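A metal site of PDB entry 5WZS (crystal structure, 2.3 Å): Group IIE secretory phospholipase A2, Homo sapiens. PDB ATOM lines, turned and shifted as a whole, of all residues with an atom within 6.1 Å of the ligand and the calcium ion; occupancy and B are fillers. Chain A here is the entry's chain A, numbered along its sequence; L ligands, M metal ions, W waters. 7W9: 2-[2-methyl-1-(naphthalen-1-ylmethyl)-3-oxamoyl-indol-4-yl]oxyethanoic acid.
Residues that only touch the ligand: Phe 5, Cys 27, Tyr 20, Gly 6, Leu 2, Ala 17, Ile 9, Asn 21, Ile 29, Lys 61, Phe 97 and Leu 18. Hydrophobic or aromatic side chains that line the ligand: Leu 2, Phe 5, Ile 9, Ala 17, Leu 18, Tyr 20, His 46 and Phe 97. The nearest printed residue that does not touch the ligand is Tyr 50 (4.6 Å).
Four residues have an atom within 4 Å of the calcium ion: Tyr 26, Gly 28, Gly 30 and Asp 47.
The calcium ion is bound by O of Tyr 26 (2.1 Å), O of Gly 28 (2.4 Å), OAN of the ligand (2.4 Å), O of Gly 30 (2.4 Å), OAS of the ligand (2.5 Å), OD1 of Asp 47 (2.7 Å) and OD2 of Asp 47 (2.9 Å).
The side-chain sulfur (SG) of Cys 43 is disulfide-bonded to the side-chain sulfur (SG) of Cys 27 (2.0 Å). N of Asp 22 lies within hydrogen-bond range of O of Cys 27 (3.0 Å). The backbone NH (N) of Phe 97 sits at hydrogen-bond distance from the side-chain sulfur (SG) of Cys 42 (3.8 Å).
An oxygen (OAS) of the ligand lies close to the backbone NH (N) of Gly 28 (2.8 Å). N of Gly 30 sits close to OAN of the ligand. The backbone carbonyl oxygen of Cys 43 is in hydrogen-bond range of a nitrogen (NAR) of the ligand, 3.0 Å away. A nitrogen (NAR) of the ligand lies close to the side-chain sulfur of Cys 43 (3.7 Å). An oxygen (OAQ) of the ligand sits at hydrogen-bond distance from a ring nitrogen (ND1) of His 46 (3.4 Å).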
ATOM      1  N   LEU A   2      -3.324  10.002   9.023  1.00  0.00           N
ATOM      2  CA  LEU A   2      -3.210  11.412   9.468  1.00  0.00           C
ATOM      3  C   LEU A   2      -2.409  12.372   8.555  1.00  0.00           C
ATOM      4  O   LEU A   2      -2.331  13.569   8.859  1.00  0.00           O
ATOM      5  CB  LEU A   2      -2.619  11.480  10.887  1.00  0.00           C
ATOM      6  CG  LEU A   2      -3.523  11.105  12.063  1.00  0.00           C
ATOM      7  CD1 LEU A   2      -2.720  11.071  13.353  1.00  0.00           C
ATOM      8  CD2 LEU A   2      -4.704  12.064  12.180  1.00  0.00           C
ATOM      9  N   VAL A   3      -1.854  11.871   7.459  1.00  0.00           N
ATOM     10  CA  VAL A   3      -0.840  12.628   6.685  1.00  0.00           C
ATOM     11  C   VAL A   3      -1.432  13.891   6.041  1.00  0.00           C
ATOM     12  O   VAL A   3      -0.877  14.983   6.193  1.00  0.00           O
ATOM     13  CB  VAL A   3      -0.155  11.736   5.607  1.00  0.00           C
ATOM     14  CG1 VAL A   3       0.905  12.532   4.833  1.00  0.00           C
ATOM     15  CG2 VAL A   3       0.470  10.493   6.255  1.00  0.00           C
ATOM     16  N   PHE A   5      -4.313  15.504   6.737  1.00  0.00           N
ATOM     17  CA  PHE A   5      -4.810  16.461   7.753  1.00  0.00           C
ATOM     18  C   PHE A   5      -3.680  17.302   8.359  1.00  0.00           C
ATOM     19  O   PHE A   5      -3.789  18.516   8.451  1.00  0.00           O
ATOM     20  CB  PHE A   5      -5.586  15.700   8.833  1.00  0.00           C
ATOM     21  CG  PHE A   5      -6.266  16.577   9.868  1.00  0.00           C
ATOM     22  CD1 PHE A   5      -6.809  17.834   9.551  1.00  0.00           C
ATOM     23  CD2 PHE A   5      -6.388  16.123  11.167  1.00  0.00           C
ATOM     24  CE1 PHE A   5      -7.423  18.599  10.531  1.00  0.00           C
ATOM     25  CE2 PHE A   5      -7.011  16.889  12.144  1.00  0.00           C
ATOM     26  CZ  PHE A   5      -7.522  18.130  11.824  1.00  0.00           C
ATOM     27  N   GLY A   6      -2.576  16.638   8.699  1.00  0.00           N
ATOM     28  CA  GLY A   6      -1.354  17.293   9.143  1.00  0.00           C
ATOM     29  C   GLY A   6      -0.833  18.299   8.156  1.00  0.00           C
ATOM     30  O   GLY A   6      -0.426  19.405   8.539  1.00  0.00           O
ATOM     31  N   VAL A   7      -0.850  17.940   6.868  1.00  0.00           N
ATOM     32  CA  VAL A   7      -0.444  18.875   5.834  1.00  0.00           C
ATOM     33  C   VAL A   7      -1.410  20.066   5.786  1.00  0.00           C
ATOM     34  O   VAL A   7      -0.983  21.213   5.716  1.00  0.00           O
ATOM     35  CB  VAL A   7      -0.300  18.206   4.436  1.00  0.00           C
ATOM     36  CG1 VAL A   7      -0.035  19.241   3.339  1.00  0.00           C
ATOM     37  CG2 VAL A   7       0.818  17.160   4.443  1.00  0.00           C
ATOM     38  N   ILE A   9      -3.315  21.237   8.222  1.00  0.00           N
ATOM     39  CA  ILE A   9      -3.110  22.065   9.425  1.00  0.00           C
ATOM     40  C   ILE A   9      -1.920  23.003   9.250  1.00  0.00           C
ATOM     41  O   ILE A   9      -2.052  24.227   9.462  1.00  0.00           O
ATOM     42  CB  ILE A   9      -2.935  21.201  10.691  1.00  0.00           C
ATOM     43  CG1 ILE A   9      -4.273  20.523  11.050  1.00  0.00           C
ATOM     44  CG2 ILE A   9      -2.478  22.054  11.879  1.00  0.00           C
ATOM     45  CD1 ILE A   9      -4.108  19.285  11.876  1.00  0.00           C
ATOM     46  N   ALA A  17       1.697  20.180  12.752  1.00  0.00           N
ATOM     47  CA  ALA A  17       0.551  19.421  13.275  1.00  0.00           C
ATOM     48  C   ALA A  17       0.793  18.810  14.661  1.00  0.00           C
ATOM     49  O   ALA A  17      -0.162  18.480  15.372  1.00  0.00           O
ATOM     50  CB  ALA A  17       0.165  18.326  12.288  1.00  0.00           C
ATOM     51  N   LEU A  18       2.069  18.638  15.022  1.00  0.00           N
ATOM     52  CA  LEU A  18       2.489  18.248  16.367  1.00  0.00           C
ATOM     53  C   LEU A  18       2.035  19.231  17.443  1.00  0.00           C
ATOM     54  O   LEU A  18       1.775  18.812  18.570  1.00  0.00           O
ATOM     55  CB  LEU A  18       4.017  18.112  16.457  1.00  0.00           C
ATOM     56  CG  LEU A  18       4.748  17.106  15.552  1.00  0.00           C
ATOM     57  CD1 LEU A  18       6.201  16.981  15.991  1.00  0.00           C
ATOM     58  CD2 LEU A  18       4.062  15.749  15.536  1.00  0.00           C
ATOM     59  N   TYR A  20      -0.794  20.697  17.569  1.00  0.00           N
ATOM     60  CA  TYR A  20      -2.199  20.406  17.857  1.00  0.00           C
ATOM     61  C   TYR A  20      -2.411  18.975  18.342  1.00  0.00           C
ATOM     62  O   TYR A  20      -3.540  18.564  18.525  1.00  0.00           O
ATOM     63  CB  TYR A  20      -3.051  20.677  16.623  1.00  0.00           C
ATOM     64  CG  TYR A  20      -3.107  22.143  16.265  1.00  0.00           C
ATOM     65  CD1 TYR A  20      -2.120  22.723  15.450  1.00  0.00           C
ATOM     66  CD2 TYR A  20      -4.115  22.962  16.760  1.00  0.00           C
ATOM     67  CE1 TYR A  20      -2.166  24.061  15.131  1.00  0.00           C
ATOM     68  CE2 TYR A  20      -4.163  24.307  16.447  1.00  0.00           C
ATOM     69  CZ  TYR A  20      -3.187  24.860  15.629  1.00  0.00           C
ATOM     70  OH  TYR A  20      -3.236  26.191  15.317  1.00  0.00           O
ATOM     71  N   ASN A  21      -1.327  18.232  18.550  1.00  0.00           N
ATOM     72  CA  ASN A  21      -1.420  16.872  19.098  1.00  0.00           C
ATOM     73  C   ASN A  21      -1.384  16.992  20.613  1.00  0.00           C
ATOM     74  O   ASN A  21      -0.532  17.695  21.169  1.00  0.00           O
ATOM     75  CB  ASN A  21      -0.261  16.021  18.592  1.00  0.00           C
ATOM     76  CG  ASN A  21      -0.349  14.574  19.055  1.00  0.00           C
ATOM     77  OD1 ASN A  21       0.576  14.076  19.707  1.00  0.00           O
ATOM     78  ND2 ASN A  21      -1.442  13.884  18.720  1.00  0.00           N
ATOM     79  N   ASP A  22      -2.326  16.314  21.260  1.00  0.00           N
ATOM     80  CA  ASP A  22      -2.547  16.394  22.713  1.00  0.00           C
ATOM     81  C   ASP A  22      -2.804  17.808  23.211  1.00  0.00           C
ATOM     82  O   ASP A  22      -2.573  18.095  24.399  1.00  0.00           O
ATOM     83  CB  ASP A  22      -1.389  15.762  23.494  1.00  0.00           C
ATOM     84  CG  ASP A  22      -1.190  14.333  23.150  1.00  0.00           C
ATOM     85  OD1 ASP A  22      -2.164  13.668  22.729  1.00  0.00           O
ATOM     86  OD2 ASP A  22      -0.051  13.862  23.314  1.00  0.00           O
ATOM     87  N   CYS A  25      -7.978  19.173  25.888  1.00  0.00           N
ATOM     88  CA  CYS A  25      -8.701  17.966  26.260  1.00  0.00           C
ATOM     89  C   CYS A  25      -9.276  17.192  25.085  1.00  0.00           C
ATOM     90  O   CYS A  25      -9.708  16.062  25.289  1.00  0.00           O
ATOM     91  CB  CYS A  25      -9.787  18.345  27.271  1.00  0.00           C
ATOM     92  SG  CYS A  25      -9.069  18.931  28.837  1.00  0.00           S
ATOM     93  N   TYR A  26      -9.298  17.770  23.879  1.00  0.00           N
ATOM     94  CA  TYR A  26      -9.881  17.082  22.713  1.00  0.00           C
ATOM     95  C   TYR A  26      -8.958  16.818  21.524  1.00  0.00           C
ATOM     96  O   TYR A  26      -9.220  15.895  20.780  1.00  0.00           O
ATOM     97  CB  TYR A  26     -11.168  17.792  22.266  1.00  0.00           C
ATOM     98  CG  TYR A  26     -12.289  17.456  23.195  1.00  0.00           C
ATOM     99  CD1 TYR A  26     -13.008  16.282  23.039  1.00  0.00           C
ATOM    100  CD2 TYR A  26     -12.574  18.272  24.279  1.00  0.00           C
ATOM    101  CE1 TYR A  26     -14.018  15.931  23.927  1.00  0.00           C
ATOM    102  CE2 TYR A  26     -13.586  17.942  25.173  1.00  0.00           C
ATOM    103  CZ  TYR A  26     -14.298  16.761  24.997  1.00  0.00           C
ATOM    104  OH  TYR A  26     -15.300  16.416  25.864  1.00  0.00           O
ATOM    105  N   CYS A  27      -7.886  17.587  21.351  1.00  0.00           N
ATOM    106  CA  CYS A  27      -7.021  17.405  20.191  1.00  0.00           C
ATOM    107  C   CYS A  27      -6.056  16.217  20.418  1.00  0.00           C
ATOM    108  O   CYS A  27      -5.302  16.203  21.381  1.00  0.00           O
ATOM    109  CB  CYS A  27      -6.248  18.667  19.896  1.00  0.00           C
ATOM    110  SG  CYS A  27      -7.250  20.156  19.733  1.00  0.00           S
ATOM    111  N   GLY A  28      -6.102  15.249  19.513  1.00  0.00           N
ATOM    112  CA  GLY A  28      -5.403  13.965  19.692  1.00  0.00           C
ATOM    113  C   GLY A  28      -6.470  12.897  19.804  1.00  0.00           C
ATOM    114  O   GLY A  28      -7.653  13.215  19.705  1.00  0.00           O
ATOM    115  N   ILE A  29      -6.072  11.647  20.023  1.00  0.00           N
ATOM    116  CA  ILE A  29      -7.048  10.550  20.026  1.00  0.00           C
ATOM    117  C   ILE A  29      -8.045  10.692  21.192  1.00  0.00           C
ATOM    118  O   ILE A  29      -7.657  11.030  22.308  1.00  0.00           O
ATOM    119  CB  ILE A  29      -6.397   9.139  20.026  1.00  0.00           C
ATOM    120  CG1 ILE A  29      -5.488   8.913  21.258  1.00  0.00           C
ATOM    121  CG2 ILE A  29      -5.614   8.917  18.732  1.00  0.00           C
ATOM    122  CD1 ILE A  29      -5.575   7.496  21.810  1.00  0.00           C
ATOM    123  N   GLY A  30      -9.328  10.461  20.897  1.00  0.00           N
ATOM    124  CA  GLY A  30     -10.376  10.568  21.904  1.00  0.00           C
ATOM    125  C   GLY A  30     -10.552  11.991  22.415  1.00  0.00           C
ATOM    126  O   GLY A  30     -10.459  12.951  21.657  1.00  0.00           O
ATOM    127  N   GLY A  31     -10.761  12.117  23.727  1.00  0.00           N
ATOM    128  CA  GLY A  31     -11.043  13.394  24.357  1.00  0.00           C
ATOM    129  C   GLY A  31     -12.278  13.284  25.228  1.00  0.00           C
ATOM    130  O   GLY A  31     -13.124  12.423  25.005  1.00  0.00           O
ATOM    131  N   CYS A  42     -12.638  23.359  18.430  1.00  0.00           N
ATOM    132  CA  CYS A  42     -12.419  22.876  17.061  1.00  0.00           C
ATOM    133  C   CYS A  42     -12.268  21.377  17.040  1.00  0.00           C
ATOM    134  O   CYS A  42     -12.867  20.703  16.207  1.00  0.00           O
ATOM    135  CB  CYS A  42     -11.174  23.492  16.422  1.00  0.00           C
ATOM    136  SG  CYS A  42     -11.048  25.291  16.434  1.00  0.00           S
ATOM    137  N   CYS A  43     -11.455  20.855  17.962  1.00  0.00           N
ATOM    138  CA  CYS A  43     -11.214  19.416  18.055  1.00  0.00           C
ATOM    139  C   CYS A  43     -12.416  18.625  18.550  1.00  0.00           C
ATOM    140  O   CYS A  43     -12.662  17.507  18.076  1.00  0.00           O
ATOM    141  CB  CYS A  43      -9.996  19.136  18.934  1.00  0.00           C
ATOM    142  SG  CYS A  43      -8.462  19.709  18.169  1.00  0.00           S
ATOM    143  N   HIS A  44     -13.161  19.186  19.506  1.00  0.00           N
ATOM    144  CA  HIS A  44     -14.438  18.612  19.951  1.00  0.00           C
ATOM    145  C   HIS A  44     -15.421  18.496  18.774  1.00  0.00           C
ATOM    146  O   HIS A  44     -15.997  17.433  18.538  1.00  0.00           O
ATOM    147  CB  HIS A  44     -15.052  19.443  21.087  1.00  0.00           C
ATOM    148  CG  HIS A  44     -16.406  18.988  21.528  1.00  0.00           C
ATOM    149  ND1 HIS A  44     -17.569  19.475  20.970  1.00  0.00           N
ATOM    150  CD2 HIS A  44     -16.791  18.114  22.485  1.00  0.00           C
ATOM    151  CE1 HIS A  44     -18.609  18.908  21.554  1.00  0.00           C
ATOM    152  NE2 HIS A  44     -18.168  18.078  22.480  1.00  0.00           N
ATOM    153  N   HIS A  46     -14.602  18.513  15.599  1.00  0.00           N
ATOM    154  CA  HIS A  46     -13.988  17.585  14.648  1.00  0.00           C
ATOM    155  C   HIS A  46     -14.267  16.128  15.019  1.00  0.00           C
ATOM    156  O   HIS A  46     -14.614  15.323  14.148  1.00  0.00           O
ATOM    157  CB  HIS A  46     -12.478  17.823  14.559  1.00  0.00           C
ATOM    158  CG  HIS A  46     -11.818  17.081  13.428  1.00  0.00           C
ATOM    159  ND1 HIS A  46     -11.062  15.949  13.622  1.00  0.00           N
ATOM    160  CD2 HIS A  46     -11.846  17.296  12.091  1.00  0.00           C
ATOM    161  CE1 HIS A  46     -10.638  15.491  12.455  1.00  0.00           C
ATOM    162  NE2 HIS A  46     -11.107  16.288  11.513  1.00  0.00           N
ATOM    163  N   ASP A  47     -14.130  15.799  16.303  1.00  0.00           N
ATOM    164  CA  ASP A  47     -14.543  14.481  16.830  1.00  0.00           C
ATOM    165  C   ASP A  47     -16.008  14.170  16.524  1.00  0.00           C
ATOM    166  O   ASP A  47     -16.337  13.051  16.102  1.00  0.00           O
ATOM    167  CB  ASP A  47     -14.361  14.429  18.353  1.00  0.00           C
ATOM    168  CG  ASP A  47     -12.895  14.323  18.789  1.00  0.00           C
ATOM    169  OD1 ASP A  47     -11.955  14.361  17.956  1.00  0.00           O
ATOM    170  OD2 ASP A  47     -12.692  14.201  20.013  1.00  0.00           O
ATOM    171  N   TYR A  50     -16.326  13.403  12.769  1.00  0.00           N
ATOM    172  CA  TYR A  50     -15.927  12.025  12.473  1.00  0.00           C
ATOM    173  C   TYR A  50     -16.987  10.990  12.917  1.00  0.00           C
ATOM    174  O   TYR A  50     -17.274  10.040  12.180  1.00  0.00           O
ATOM    175  CB  TYR A  50     -14.523  11.713  13.045  1.00  0.00           C
ATOM    176  CG  TYR A  50     -13.336  12.095  12.145  1.00  0.00           C
ATOM    177  CD1 TYR A  50     -13.412  13.105  11.188  1.00  0.00           C
ATOM    178  CD2 TYR A  50     -12.115  11.434  12.287  1.00  0.00           C
ATOM    179  CE1 TYR A  50     -12.318  13.417  10.385  1.00  0.00           C
ATOM    180  CE2 TYR A  50     -11.017  11.745  11.501  1.00  0.00           C
ATOM    181  CZ  TYR A  50     -11.116  12.736  10.544  1.00  0.00           C
ATOM    182  OH  TYR A  50     -10.012  13.026   9.768  1.00  0.00           O
ATOM    183  N   LYS A  61     -11.102   8.058  10.080  1.00  0.00           N
ATOM    184  CA  LYS A  61      -9.740   7.833  10.604  1.00  0.00           C
ATOM    185  C   LYS A  61      -8.773   7.292   9.570  1.00  0.00           C
ATOM    186  O   LYS A  61      -7.587   7.526   9.694  1.00  0.00           O
ATOM    187  CB  LYS A  61      -9.757   6.875  11.796  1.00  0.00           C
ATOM    188  CG  LYS A  61     -10.275   7.510  13.073  1.00  0.00           C
ATOM    189  CD  LYS A  61     -10.801   6.455  14.038  1.00  0.00           C
ATOM    190  CE  LYS A  61     -10.953   7.033  15.443  1.00  0.00           C
ATOM    191  NZ  LYS A  61     -12.041   6.344  16.195  1.00  0.00           N
ATOM    192  N   ALA A  93     -12.100  22.017  10.580  1.00  0.00           N
ATOM    193  CA  ALA A  93     -11.157  22.035  11.701  1.00  0.00           C
ATOM    194  C   ALA A  93      -9.911  22.884  11.475  1.00  0.00           C
ATOM    195  O   ALA A  93      -9.468  23.570  12.386  1.00  0.00           O
ATOM    196  CB  ALA A  93     -10.751  20.610  12.073  1.00  0.00           C
ATOM    197  N   PHE A  97      -8.924  26.166  13.454  1.00  0.00           N
ATOM    198  CA  PHE A  97      -7.609  26.421  14.068  1.00  0.00           C
ATOM    199  C   PHE A  97      -7.033  27.786  13.659  1.00  0.00           C
ATOM    200  O   PHE A  97      -6.594  28.557  14.535  1.00  0.00           O
ATOM    201  CB  PHE A  97      -6.575  25.340  13.721  1.00  0.00           C
ATOM    202  CG  PHE A  97      -6.887  23.951  14.250  1.00  0.00           C
ATOM    203  CD1 PHE A  97      -7.594  23.741  15.439  1.00  0.00           C
ATOM    204  CD2 PHE A  97      -6.411  22.839  13.557  1.00  0.00           C
ATOM    205  CE1 PHE A  97      -7.831  22.438  15.894  1.00  0.00           C
ATOM    206  CE2 PHE A  97      -6.647  21.550  14.012  1.00  0.00           C
ATOM    207  CZ  PHE A  97      -7.349  21.353  15.188  1.00  0.00           C
HETATM  208  OAM 7W9 L   1      -9.859  10.393  17.028  1.00  0.00           O
HETATM  209  CAL 7W9 L   1      -9.664  11.629  17.080  1.00  0.00           C
HETATM  210  OAN 7W9 L   1      -9.805  12.334  18.101  1.00  0.00           O
HETATM  211  CAK 7W9 L   1      -9.248  12.353  15.780  1.00  0.00           C
HETATM  212  OAJ 7W9 L   1      -8.367  13.468  16.065  1.00  0.00           O
HETATM  213  CAA 7W9 L   1      -6.998  13.376  16.043  1.00  0.00           C
HETATM  214  CAB 7W9 L   1      -6.354  12.130  16.117  1.00  0.00           C
HETATM  215  CAC 7W9 L   1      -4.970  12.086  16.091  1.00  0.00           C
HETATM  216  CAD 7W9 L   1      -4.276  13.293  16.002  1.00  0.00           C
HETATM  217  CAE 7W9 L   1      -4.930  14.470  15.942  1.00  0.00           C
HETATM  218  CAF 7W9 L   1      -6.274  14.539  15.952  1.00  0.00           C
HETATM  219  CAI 7W9 L   1      -6.596  15.863  15.887  1.00  0.00           C
HETATM  220  CAO 7W9 L   1      -7.832  16.421  15.886  1.00  0.00           C
HETATM  221  OAQ 7W9 L   1      -8.241  17.178  15.006  1.00  0.00           O
HETATM  222  CAP 7W9 L   1      -8.785  16.106  17.057  1.00  0.00           C
HETATM  223  OAS 7W9 L   1      -8.455  15.382  17.983  1.00  0.00           O
HETATM  224  NAR 7W9 L   1      -9.982  16.623  16.945  1.00  0.00           N
HETATM  225  CAH 7W9 L   1      -5.451  16.544  15.819  1.00  0.00           C
HETATM  226  CBE 7W9 L   1      -5.332  18.073  15.719  1.00  0.00           C
HETATM  227  NAG 7W9 L   1      -4.400  15.702  15.838  1.00  0.00           N
HETATM  228  CAT 7W9 L   1      -2.901  15.984  15.788  1.00  0.00           C
HETATM  229  CAU 7W9 L   1      -2.363  15.658  14.476  1.00  0.00           C
HETATM  230  CAZ 7W9 L   1      -1.161  14.921  14.192  1.00  0.00           C
HETATM  231  CBD 7W9 L   1      -0.316  14.348  15.165  1.00  0.00           C
HETATM  232  CBC 7W9 L   1       0.842  13.621  14.827  1.00  0.00           C
HETATM  233  CBB 7W9 L   1       1.206  13.434  13.491  1.00  0.00           C
HETATM  234  CBA 7W9 L   1       0.400  13.982  12.495  1.00  0.00           C
HETATM  235  CAY 7W9 L   1      -0.761  14.703  12.840  1.00  0.00           C
HETATM  236  CAX 7W9 L   1      -1.508  15.205  11.793  1.00  0.00           C
HETATM  237  CAW 7W9 L   1      -2.662  15.917  12.058  1.00  0.00           C
HETATM  238  CAV 7W9 L   1      -3.076  16.156  13.366  1.00  0.00           C
HETATM  239 CA    CA M   1      -9.840  14.175  19.657  1.00  0.00          CA
HETATM  240  O   HOH W   1     -12.184  10.419  15.520  1.00  0.00           O
